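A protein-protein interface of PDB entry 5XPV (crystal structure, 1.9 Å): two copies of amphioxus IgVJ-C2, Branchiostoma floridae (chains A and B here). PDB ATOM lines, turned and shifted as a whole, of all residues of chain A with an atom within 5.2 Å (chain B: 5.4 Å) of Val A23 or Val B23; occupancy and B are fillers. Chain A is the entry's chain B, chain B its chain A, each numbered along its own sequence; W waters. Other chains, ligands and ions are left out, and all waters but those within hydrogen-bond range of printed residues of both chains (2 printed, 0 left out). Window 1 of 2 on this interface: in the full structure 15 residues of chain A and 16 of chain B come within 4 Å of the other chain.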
ATOM      1  N   THR A  21      14.074  -1.940  21.588  1.00  0.00           N
ATOM      2  CA  THR A  21      14.438  -1.140  22.747  1.00  0.00           C
ATOM      3  C   THR A  21      15.919  -0.796  22.689  1.00  0.00           C
ATOM      4  O   THR A  21      16.765  -1.682  22.581  1.00  0.00           O
ATOM      5  CB  THR A  21      14.129  -1.873  24.068  1.00  0.00           C
ATOM      6  OG1 THR A  21      12.733  -2.190  24.121  1.00  0.00           O
ATOM      7  CG2 THR A  21      14.490  -0.996  25.263  1.00  0.00           C
ATOM      8  N   TYR A  22      16.231   0.492  22.761  1.00  0.00           N
ATOM      9  CA  TYR A  22      17.609   0.939  22.613  1.00  0.00           C
ATOM     10  C   TYR A  22      17.817   2.299  23.249  1.00  0.00           C
ATOM     11  O   TYR A  22      16.858   3.006  23.555  1.00  0.00           O
ATOM     12  CB  TYR A  22      17.995   0.991  21.133  1.00  0.00           C
ATOM     13  CG  TYR A  22      17.046   1.816  20.295  1.00  0.00           C
ATOM     14  CD1 TYR A  22      15.909   1.242  19.740  1.00  0.00           C
ATOM     15  CD2 TYR A  22      17.281   3.167  20.059  1.00  0.00           C
ATOM     16  CE1 TYR A  22      15.030   1.985  18.978  1.00  0.00           C
ATOM     17  CE2 TYR A  22      16.401   3.923  19.289  1.00  0.00           C
ATOM     18  CZ  TYR A  22      15.279   3.319  18.753  1.00  0.00           C
ATOM     19  OH  TYR A  22      14.392   4.041  17.985  1.00  0.00           O
ATOM     20  N   VAL A  23      19.082   2.651  23.453  1.00  0.00           N
ATOM     21  CA  VAL A  23      19.446   3.969  23.960  1.00  0.00           C
ATOM     22  C   VAL A  23      20.407   4.642  22.992  1.00  0.00           C
ATOM     23  O   VAL A  23      21.334   4.007  22.481  1.00  0.00           O
ATOM     24  CB  VAL A  23      20.105   3.885  25.364  1.00  0.00           C
ATOM     25  CG1 VAL A  23      20.679   5.237  25.773  1.00  0.00           C
ATOM     26  CG2 VAL A  23      19.101   3.414  26.379  1.00  0.00           C
ATOM     27  N   ILE A  24      20.175   5.926  22.737  1.00  0.00           N
ATOM     28  CA  ILE A  24      21.085   6.714  21.925  1.00  0.00           C
ATOM     29  C   ILE A  24      21.708   7.819  22.767  1.00  0.00           C
ATOM     30  O   ILE A  24      21.002   8.528  23.488  1.00  0.00           O
ATOM     31  CB  ILE A  24      20.361   7.345  20.712  1.00  0.00           C
ATOM     32  CG1 ILE A  24      19.711   6.263  19.848  1.00  0.00           C
ATOM     33  CG2 ILE A  24      21.333   8.178  19.890  1.00  0.00           C
ATOM     34  CD1 ILE A  24      18.886   6.812  18.689  1.00  0.00           C
ATOM     35  N   ASN A  25      23.028   7.959  22.691  1.00  0.00           N
ATOM     36  CA  ASN A  25      23.707   9.114  23.270  1.00  0.00           C
ATOM     37  C   ASN A  25      24.455   9.872  22.191  1.00  0.00           C
ATOM     38  O   ASN A  25      24.947   9.270  21.244  1.00  0.00           O
ATOM     39  CB  ASN A  25      24.689   8.698  24.373  1.00  0.00           C
ATOM     40  CG  ASN A  25      23.995   8.337  25.667  1.00  0.00           C
ATOM     41  OD1 ASN A  25      23.241   7.370  25.723  1.00  0.00           O
ATOM     42  ND2 ASN A  25      24.264   9.104  26.723  1.00  0.00           N
ATOM     43  N   TYR A  36      18.938   9.433  25.219  1.00  0.00           N
ATOM     44  CA  TYR A  36      17.589   9.131  24.773  1.00  0.00           C
ATOM     45  C   TYR A  36      17.329   7.638  24.886  1.00  0.00           C
ATOM     46  O   TYR A  36      18.091   6.831  24.365  1.00  0.00           O
ATOM     47  CB  TYR A  36      17.379   9.611  23.329  1.00  0.00           C
ATOM     48  CG  TYR A  36      16.115   9.092  22.670  1.00  0.00           C
ATOM     49  CD1 TYR A  36      14.882   9.696  22.906  1.00  0.00           C
ATOM     50  CD2 TYR A  36      16.156   8.006  21.807  1.00  0.00           C
ATOM     51  CE1 TYR A  36      13.723   9.221  22.303  1.00  0.00           C
ATOM     52  CE2 TYR A  36      15.005   7.520  21.202  1.00  0.00           C
ATOM     53  CZ  TYR A  36      13.792   8.134  21.453  1.00  0.00           C
ATOM     54  OH  TYR A  36      12.652   7.654  20.853  1.00  0.00           O
ATOM     55  N   LEU A  37      16.251   7.276  25.570  1.00  0.00           N
ATOM     56  CA  LEU A  37      15.791   5.891  25.623  1.00  0.00           C
ATOM     57  C   LEU A  37      14.584   5.766  24.699  1.00  0.00           C
ATOM     58  O   LEU A  37      13.692   6.609  24.749  1.00  0.00           O
ATOM     59  CB  LEU A  37      15.433   5.493  27.061  1.00  0.00           C
ATOM     60  CG  LEU A  37      14.660   4.192  27.279  1.00  0.00           C
ATOM     61  CD1 LEU A  37      15.469   2.997  26.812  1.00  0.00           C
ATOM     62  CD2 LEU A  37      14.281   4.045  28.750  1.00  0.00           C
ATOM     63  N   SER A  38      14.569   4.742  23.846  1.00  0.00           N
ATOM     64  CA  SER A  38      13.489   4.563  22.873  1.00  0.00           C
ATOM     65  C   SER A  38      12.121   4.624  23.550  1.00  0.00           C
ATOM     66  O   SER A  38      11.886   3.954  24.556  1.00  0.00           O
ATOM     67  CB  SER A  38      13.655   3.237  22.119  1.00  0.00           C
ATOM     68  OG  SER A  38      13.667   2.128  23.003  1.00  0.00           O
ATOM     69  N   SER A  78      26.452   7.080  20.092  1.00  0.00           N
ATOM     70  CA  SER A  78      26.619   5.700  20.533  1.00  0.00           C
ATOM     71  C   SER A  78      25.247   5.078  20.704  1.00  0.00           C
ATOM     72  O   SER A  78      24.337   5.707  21.241  1.00  0.00           O
ATOM     73  CB  SER A  78      27.395   5.618  21.851  1.00  0.00           C
ATOM     74  OG  SER A  78      28.739   6.021  21.677  1.00  0.00           O
ATOM     75  N   VAL A  79      25.092   3.844  20.245  1.00  0.00           N
ATOM     76  CA  VAL A  79      23.823   3.154  20.379  1.00  0.00           C
ATOM     77  C   VAL A  79      24.009   1.907  21.225  1.00  0.00           C
ATOM     78  O   VAL A  79      24.954   1.152  21.014  1.00  0.00           O
ATOM     79  CB  VAL A  79      23.252   2.765  19.001  1.00  0.00           C
ATOM     80  CG1 VAL A  79      21.990   1.931  19.151  1.00  0.00           C
ATOM     81  CG2 VAL A  79      22.981   4.015  18.182  1.00  0.00           C
ATOM     82  N   ILE A  80      23.125   1.703  22.193  1.00  0.00           N
ATOM     83  CA  ILE A  80      23.094   0.443  22.924  1.00  0.00           C
ATOM     84  C   ILE A  80      21.746  -0.222  22.690  1.00  0.00           C
ATOM     85  O   ILE A  80      20.704   0.359  22.986  1.00  0.00           O
ATOM     86  CB  ILE A  80      23.323   0.619  24.448  1.00  0.00           C
ATOM     87  CG1 ILE A  80      24.808   0.821  24.767  1.00  0.00           C
ATOM     88  CG2 ILE A  80      22.860  -0.625  25.198  1.00  0.00           C
ATOM     89  CD1 ILE A  80      25.373   2.141  24.359  1.00  0.00           C
ATOM     90  N   GLU A  81      21.773  -1.433  22.145  1.00  0.00           N
ATOM     91  CA  GLU A  81      20.552  -2.211  21.953  1.00  0.00           C
ATOM     92  C   GLU A  81      20.258  -3.062  23.180  1.00  0.00           C
ATOM     93  O   GLU A  81      21.161  -3.671  23.757  1.00  0.00           O
ATOM     94  CB  GLU A  81      20.667  -3.089  20.709  1.00  0.00           C
ATOM     95  CG  GLU A  81      20.884  -2.291  19.440  1.00  0.00           C
ATOM     96  CD  GLU A  81      20.901  -3.158  18.197  1.00  0.00           C
ATOM     97  OE1 GLU A  81      21.443  -4.285  18.260  1.00  0.00           O
ATOM     98  OE2 GLU A  81      20.357  -2.714  17.163  1.00  0.00           O
ATOM     99  N   ILE A  82      18.992  -3.098  23.579  1.00  0.00           N
ATOM    100  CA  ILE A  82      18.601  -3.806  24.789  1.00  0.00           C
ATOM    101  C   ILE A  82      17.875  -5.098  24.440  1.00  0.00           C
ATOM    102  O   ILE A  82      16.952  -5.101  23.622  1.00  0.00           O
ATOM    103  CB  ILE A  82      17.711  -2.932  25.679  1.00  0.00           C
ATOM    104  CG1 ILE A  82      18.476  -1.681  26.111  1.00  0.00           C
ATOM    105  CG2 ILE A  82      17.256  -3.698  26.913  1.00  0.00           C
ATOM    106  CD1 ILE A  82      19.611  -1.967  27.064  1.00  0.00           C
ATOM    107  N   THR B  21      16.618   5.631  36.071  1.00  0.00           N
ATOM    108  CA  THR B  21      16.613   4.826  34.857  1.00  0.00           C
ATOM    109  C   THR B  21      18.005   4.847  34.240  1.00  0.00           C
ATOM    110  O   THR B  21      18.616   5.907  34.104  1.00  0.00           O
ATOM    111  CB  THR B  21      15.579   5.341  33.834  1.00  0.00           C
ATOM    112  OG1 THR B  21      14.279   5.362  34.438  1.00  0.00           O
ATOM    113  CG2 THR B  21      15.545   4.438  32.604  1.00  0.00           C
ATOM    114  N   TYR B  22      18.507   3.673  33.874  1.00  0.00           N
ATOM    115  CA  TYR B  22      19.883   3.549  33.421  1.00  0.00           C
ATOM    116  C   TYR B  22      20.104   2.228  32.707  1.00  0.00           C
ATOM    117  O   TYR B  22      19.319   1.289  32.842  1.00  0.00           O
ATOM    118  CB  TYR B  22      20.851   3.669  34.602  1.00  0.00           C
ATOM    119  CG  TYR B  22      20.539   2.686  35.710  1.00  0.00           C
ATOM    120  CD1 TYR B  22      19.594   2.989  36.686  1.00  0.00           C
ATOM    121  CD2 TYR B  22      21.172   1.449  35.769  1.00  0.00           C
ATOM    122  CE1 TYR B  22      19.294   2.089  37.698  1.00  0.00           C
ATOM    123  CE2 TYR B  22      20.880   0.543  36.781  1.00  0.00           C
ATOM    124  CZ  TYR B  22      19.939   0.870  37.738  1.00  0.00           C
ATOM    125  OH  TYR B  22      19.638  -0.025  38.742  1.00  0.00           O
ATOM    126  N   VAL B  23      21.190   2.172  31.950  1.00  0.00           N
ATOM    127  CA  VAL B  23      21.574   0.972  31.232  1.00  0.00           C
ATOM    128  C   VAL B  23      22.982   0.566  31.654  1.00  0.00           C
ATOM    129  O   VAL B  23      23.849   1.421  31.838  1.00  0.00           O
ATOM    130  CB  VAL B  23      21.512   1.197  29.705  1.00  0.00           C
ATOM    131  CG1 VAL B  23      22.125   0.027  28.954  1.00  0.00           C
ATOM    132  CG2 VAL B  23      20.072   1.419  29.276  1.00  0.00           C
ATOM    133  N   ILE B  24      23.192  -0.734  31.841  1.00  0.00           N
ATOM    134  CA  ILE B  24      24.508  -1.269  32.135  1.00  0.00           C
ATOM    135  C   ILE B  24      24.925  -2.265  31.053  1.00  0.00           C
ATOM    136  O   ILE B  24      24.155  -3.156  30.699  1.00  0.00           O
ATOM    137  CB  ILE B  24      24.545  -1.969  33.521  1.00  0.00           C
ATOM    138  CG1 ILE B  24      24.260  -0.967  34.644  1.00  0.00           C
ATOM    139  CG2 ILE B  24      25.889  -2.661  33.732  1.00  0.00           C
ATOM    140  CD1 ILE B  24      24.076  -1.605  36.042  1.00  0.00           C
ATOM    141  N   ASN B  25      26.133  -2.101  30.520  1.00  0.00           N
ATOM    142  CA  ASN B  25      26.746  -3.110  29.660  1.00  0.00           C
ATOM    143  C   ASN B  25      28.045  -3.624  30.260  1.00  0.00           C
ATOM    144  O   ASN B  25      28.784  -2.862  30.882  1.00  0.00           O
ATOM    145  CB  ASN B  25      27.040  -2.553  28.262  1.00  0.00           C
ATOM    146  CG  ASN B  25      25.791  -2.378  27.424  1.00  0.00           C
ATOM    147  OD1 ASN B  25      24.930  -1.562  27.749  1.00  0.00           O
ATOM    148  ND2 ASN B  25      25.694  -3.132  26.328  1.00  0.00           N
ATOM    149  N   TYR B  36      21.754  -4.548  29.959  1.00  0.00           N
ATOM    150  CA  TYR B  36      20.697  -4.533  30.957  1.00  0.00           C
ATOM    151  C   TYR B  36      20.098  -3.141  31.061  1.00  0.00           C
ATOM    152  O   TYR B  36      20.827  -2.164  31.186  1.00  0.00           O
ATOM    153  CB  TYR B  36      21.244  -4.980  32.320  1.00  0.00           C
ATOM    154  CG  TYR B  36      20.347  -4.675  33.499  1.00  0.00           C
ATOM    155  CD1 TYR B  36      19.279  -5.512  33.825  1.00  0.00           C
ATOM    156  CD2 TYR B  36      20.585  -3.572  34.309  1.00  0.00           C
ATOM    157  CE1 TYR B  36      18.461  -5.239  34.914  1.00  0.00           C
ATOM    158  CE2 TYR B  36      19.772  -3.294  35.398  1.00  0.00           C
ATOM    159  CZ  TYR B  36      18.713  -4.128  35.696  1.00  0.00           C
ATOM    160  OH  TYR B  36      17.906  -3.847  36.785  1.00  0.00           O
ATOM    161  N   LEU B  37      18.773  -3.062  30.999  1.00  0.00           N
ATOM    162  CA  LEU B  37      18.053  -1.820  31.266  1.00  0.00           C
ATOM    163  C   LEU B  37      17.428  -1.911  32.649  1.00  0.00           C
ATOM    164  O   LEU B  37      16.888  -2.955  33.012  1.00  0.00           O
ATOM    165  CB  LEU B  37      16.983  -1.568  30.199  1.00  0.00           C
ATOM    166  CG  LEU B  37      15.958  -0.465  30.464  1.00  0.00           C
ATOM    167  CD1 LEU B  37      16.629   0.902  30.632  1.00  0.00           C
ATOM    168  CD2 LEU B  37      14.933  -0.433  29.333  1.00  0.00           C
ATOM    169  N   SER B  38      17.520  -0.832  33.424  1.00  0.00           N
ATOM    170  CA  SER B  38      17.039  -0.833  34.807  1.00  0.00           C
ATOM    171  C   SER B  38      15.604  -1.351  34.903  1.00  0.00           C
ATOM    172  O   SER B  38      14.737  -0.947  34.139  1.00  0.00           O
ATOM    173  CB  SER B  38      17.137   0.572  35.413  1.00  0.00           C
ATOM    174  OG  SER B  38      16.481   1.538  34.605  1.00  0.00           O
ATOM    175  N   SER B  78      30.096  -0.415  31.419  1.00  0.00           N
ATOM    176  CA  SER B  78      29.761   0.934  30.981  1.00  0.00           C
ATOM    177  C   SER B  78      28.351   1.257  31.439  1.00  0.00           C
ATOM    178  O   SER B  78      27.445   0.440  31.286  1.00  0.00           O
ATOM    179  CB  SER B  78      29.862   1.076  29.455  1.00  0.00           C
ATOM    180  OG  SER B  78      31.202   0.937  29.018  1.00  0.00           O
ATOM    181  N   VAL B  79      28.170   2.448  31.998  1.00  0.00           N
ATOM    182  CA  VAL B  79      26.870   2.878  32.495  1.00  0.00           C
ATOM    183  C   VAL B  79      26.351   4.083  31.710  1.00  0.00           C
ATOM    184  O   VAL B  79      27.103   5.011  31.426  1.00  0.00           O
ATOM    185  CB  VAL B  79      26.946   3.232  33.994  1.00  0.00           C
ATOM    186  CG1 VAL B  79      25.661   3.885  34.462  1.00  0.00           C
ATOM    187  CG2 VAL B  79      27.234   1.981  34.807  1.00  0.00           C
ATOM    188  N   ILE B  80      25.077   4.055  31.337  1.00  0.00           N
ATOM    189  CA  ILE B  80      24.441   5.225  30.739  1.00  0.00           C
ATOM    190  C   ILE B  80      23.202   5.585  31.547  1.00  0.00           C
ATOM    191  O   ILE B  80      22.274   4.784  31.659  1.00  0.00           O
ATOM    192  CB  ILE B  80      24.029   5.006  29.268  1.00  0.00           C
ATOM    193  CG1 ILE B  80      25.243   5.068  28.338  1.00  0.00           C
ATOM    194  CG2 ILE B  80      23.055   6.092  28.835  1.00  0.00           C
ATOM    195  CD1 ILE B  80      26.107   3.837  28.345  1.00  0.00           C
ATOM    196  N   GLU B  81      23.200   6.781  32.124  1.00  0.00           N
ATOM    197  CA  GLU B  81      22.037   7.264  32.854  1.00  0.00           C
ATOM    198  C   GLU B  81      21.048   7.946  31.917  1.00  0.00           C
ATOM    199  O   GLU B  81      21.440   8.705  31.031  1.00  0.00           O
ATOM    200  CB  GLU B  81      22.461   8.232  33.959  1.00  0.00           C
ATOM    201  CG  GLU B  81      23.207   7.564  35.095  1.00  0.00           C
ATOM    202  CD  GLU B  81      23.666   8.557  36.142  1.00  0.00           C
ATOM    203  OE1 GLU B  81      23.832   9.754  35.812  1.00  0.00           O
ATOM    204  OE2 GLU B  81      23.855   8.137  37.298  1.00  0.00           O
ATOM    205  N   ILE B  82      19.764   7.671  32.120  1.00  0.00           N
ATOM    206  CA  ILE B  82      18.716   8.275  31.306  1.00  0.00           C
ATOM    207  C   ILE B  82      18.055   9.439  32.037  1.00  0.00           C
ATOM    208  O   ILE B  82      17.720   9.327  33.215  1.00  0.00           O
ATOM    209  CB  ILE B  82      17.635   7.241  30.927  1.00  0.00           C
ATOM    210  CG1 ILE B  82      18.258   6.027  30.224  1.00  0.00           C
ATOM    211  CG2 ILE B  82      16.571   7.883  30.053  1.00  0.00           C
ATOM    212  CD1 ILE B  82      19.069   6.378  28.992  1.00  0.00           C
HETATM  213  O   HOH W   1      23.878  -3.877  23.998  1.00  0.00           O
HETATM  214  O   HOH W   2      23.686   9.566  29.584  1.00  0.00           O
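The backbone carbonyl oxygen (O) of Thr B21 lies within hydrogen-bond range of the backbone NH (N) of Ile B82, 2.9 Å away. N of Val B23 sits at hydrogen-bond distance from O of Ile B80 (2.8 Å). O of Asn B25 sits at hydrogen-bond distance from N of Ser B78. The backbone carbonyl oxygen (O) of Thr A21 is in hydrogen-bond range of the backbone NH (N) of Ile A82. The backbone NH (N) of Val A23 sits at hydrogen-bond distance from the backbone carbonyl oxygen (O) of Ile A80 (2.8 Å). O of Asn A25 is in hydrogen-bond range of N of Ser A78, 2.9 Å away.
Of chain B, only Val B23, Ile B80 and Ile B82 come within 4 Å of Val A23. Ile A24 touches none of the printed residues of chain B. Printed residues of chain B within 4 Å of Leu A37: Ile B82. Printed residues of chain B within 4 Å of Ile A80: Val B23 and Asn B25. Thr B21 touches none of the printed residues of chain A. Val B23 touches just these residues of chain A: Val A23 (3.6 Å), Ile A80 (3.9 Å) and Ile A82 (3.7 Å). Of the printed residues of chain A, Leu B37 touches Ile A82 (3.9 Å). Printed residues of chain A within 4 Å of Ile B80: Val A23 and Asn A25. The nearest printed residue of chain A that does not touch Val B23 is Leu A37 (5.5 Å).
Water W1 lies within hydrogen-bond range of the backbone carbonyl oxygen of Glu A81 (2.7 Å) and the side-chain amide nitrogen of Asn B25 (3.0 Å). Water W2 bridges O of Glu B81 (2.8 Å) and ND2 of Asn A25 (3.0 Å).
Hydrophobic or aromatic side chains of chain A within 4 Å of the printed part of chain B: Val A23, Leu A37, Ile A80 and Ile A82. Hydrophobic or aromatic side chains of chain B within 4 Å of the printed part of chain A: Val B23, Leu B37, Ile B80 and Ile B82. Among the printed residues, 9 pairs touch across the chains. Among the printed residues, no Asp or Glu carboxylate lies within 4 Å of a Lys or Arg side-chain nitrogen of the other chain.
Val B23 touches its own counterpart, Val A23. Val A23 touches Ile B82, and with the chains exchanged Ile A82 touches Val B23. Asn A25 touches Ile B80, and with the chains exchanged Ile A80 touches Asn B25. Leu A37 touches Ile B82, and with the chains exchanged Ile A82 touches Leu B37. 13 positions are printed for both chains.
Val B23 touches Val A23 (CG2 to CG2, 3.6 Å). CG2 of Ile B80 touches CG1 of Val A23, 3.97 Å away. CG1 of Val A23 touches CD1 of Ile B82, 3.8 Å away. Asn A25 touches Ile B80. CG2 of Ile B82 touches CB of Leu A37 (3.99 Å). Val B23 touches Ile A80. Asn B25 touches Ile A80 (OD1 to CG2, 3.4 Å). CD1 of Ile A82 touches CG1 of Val B23, at 3.7 Å. Ile A82 touches Leu B37 (CG2 to CB, 3.9 Å).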
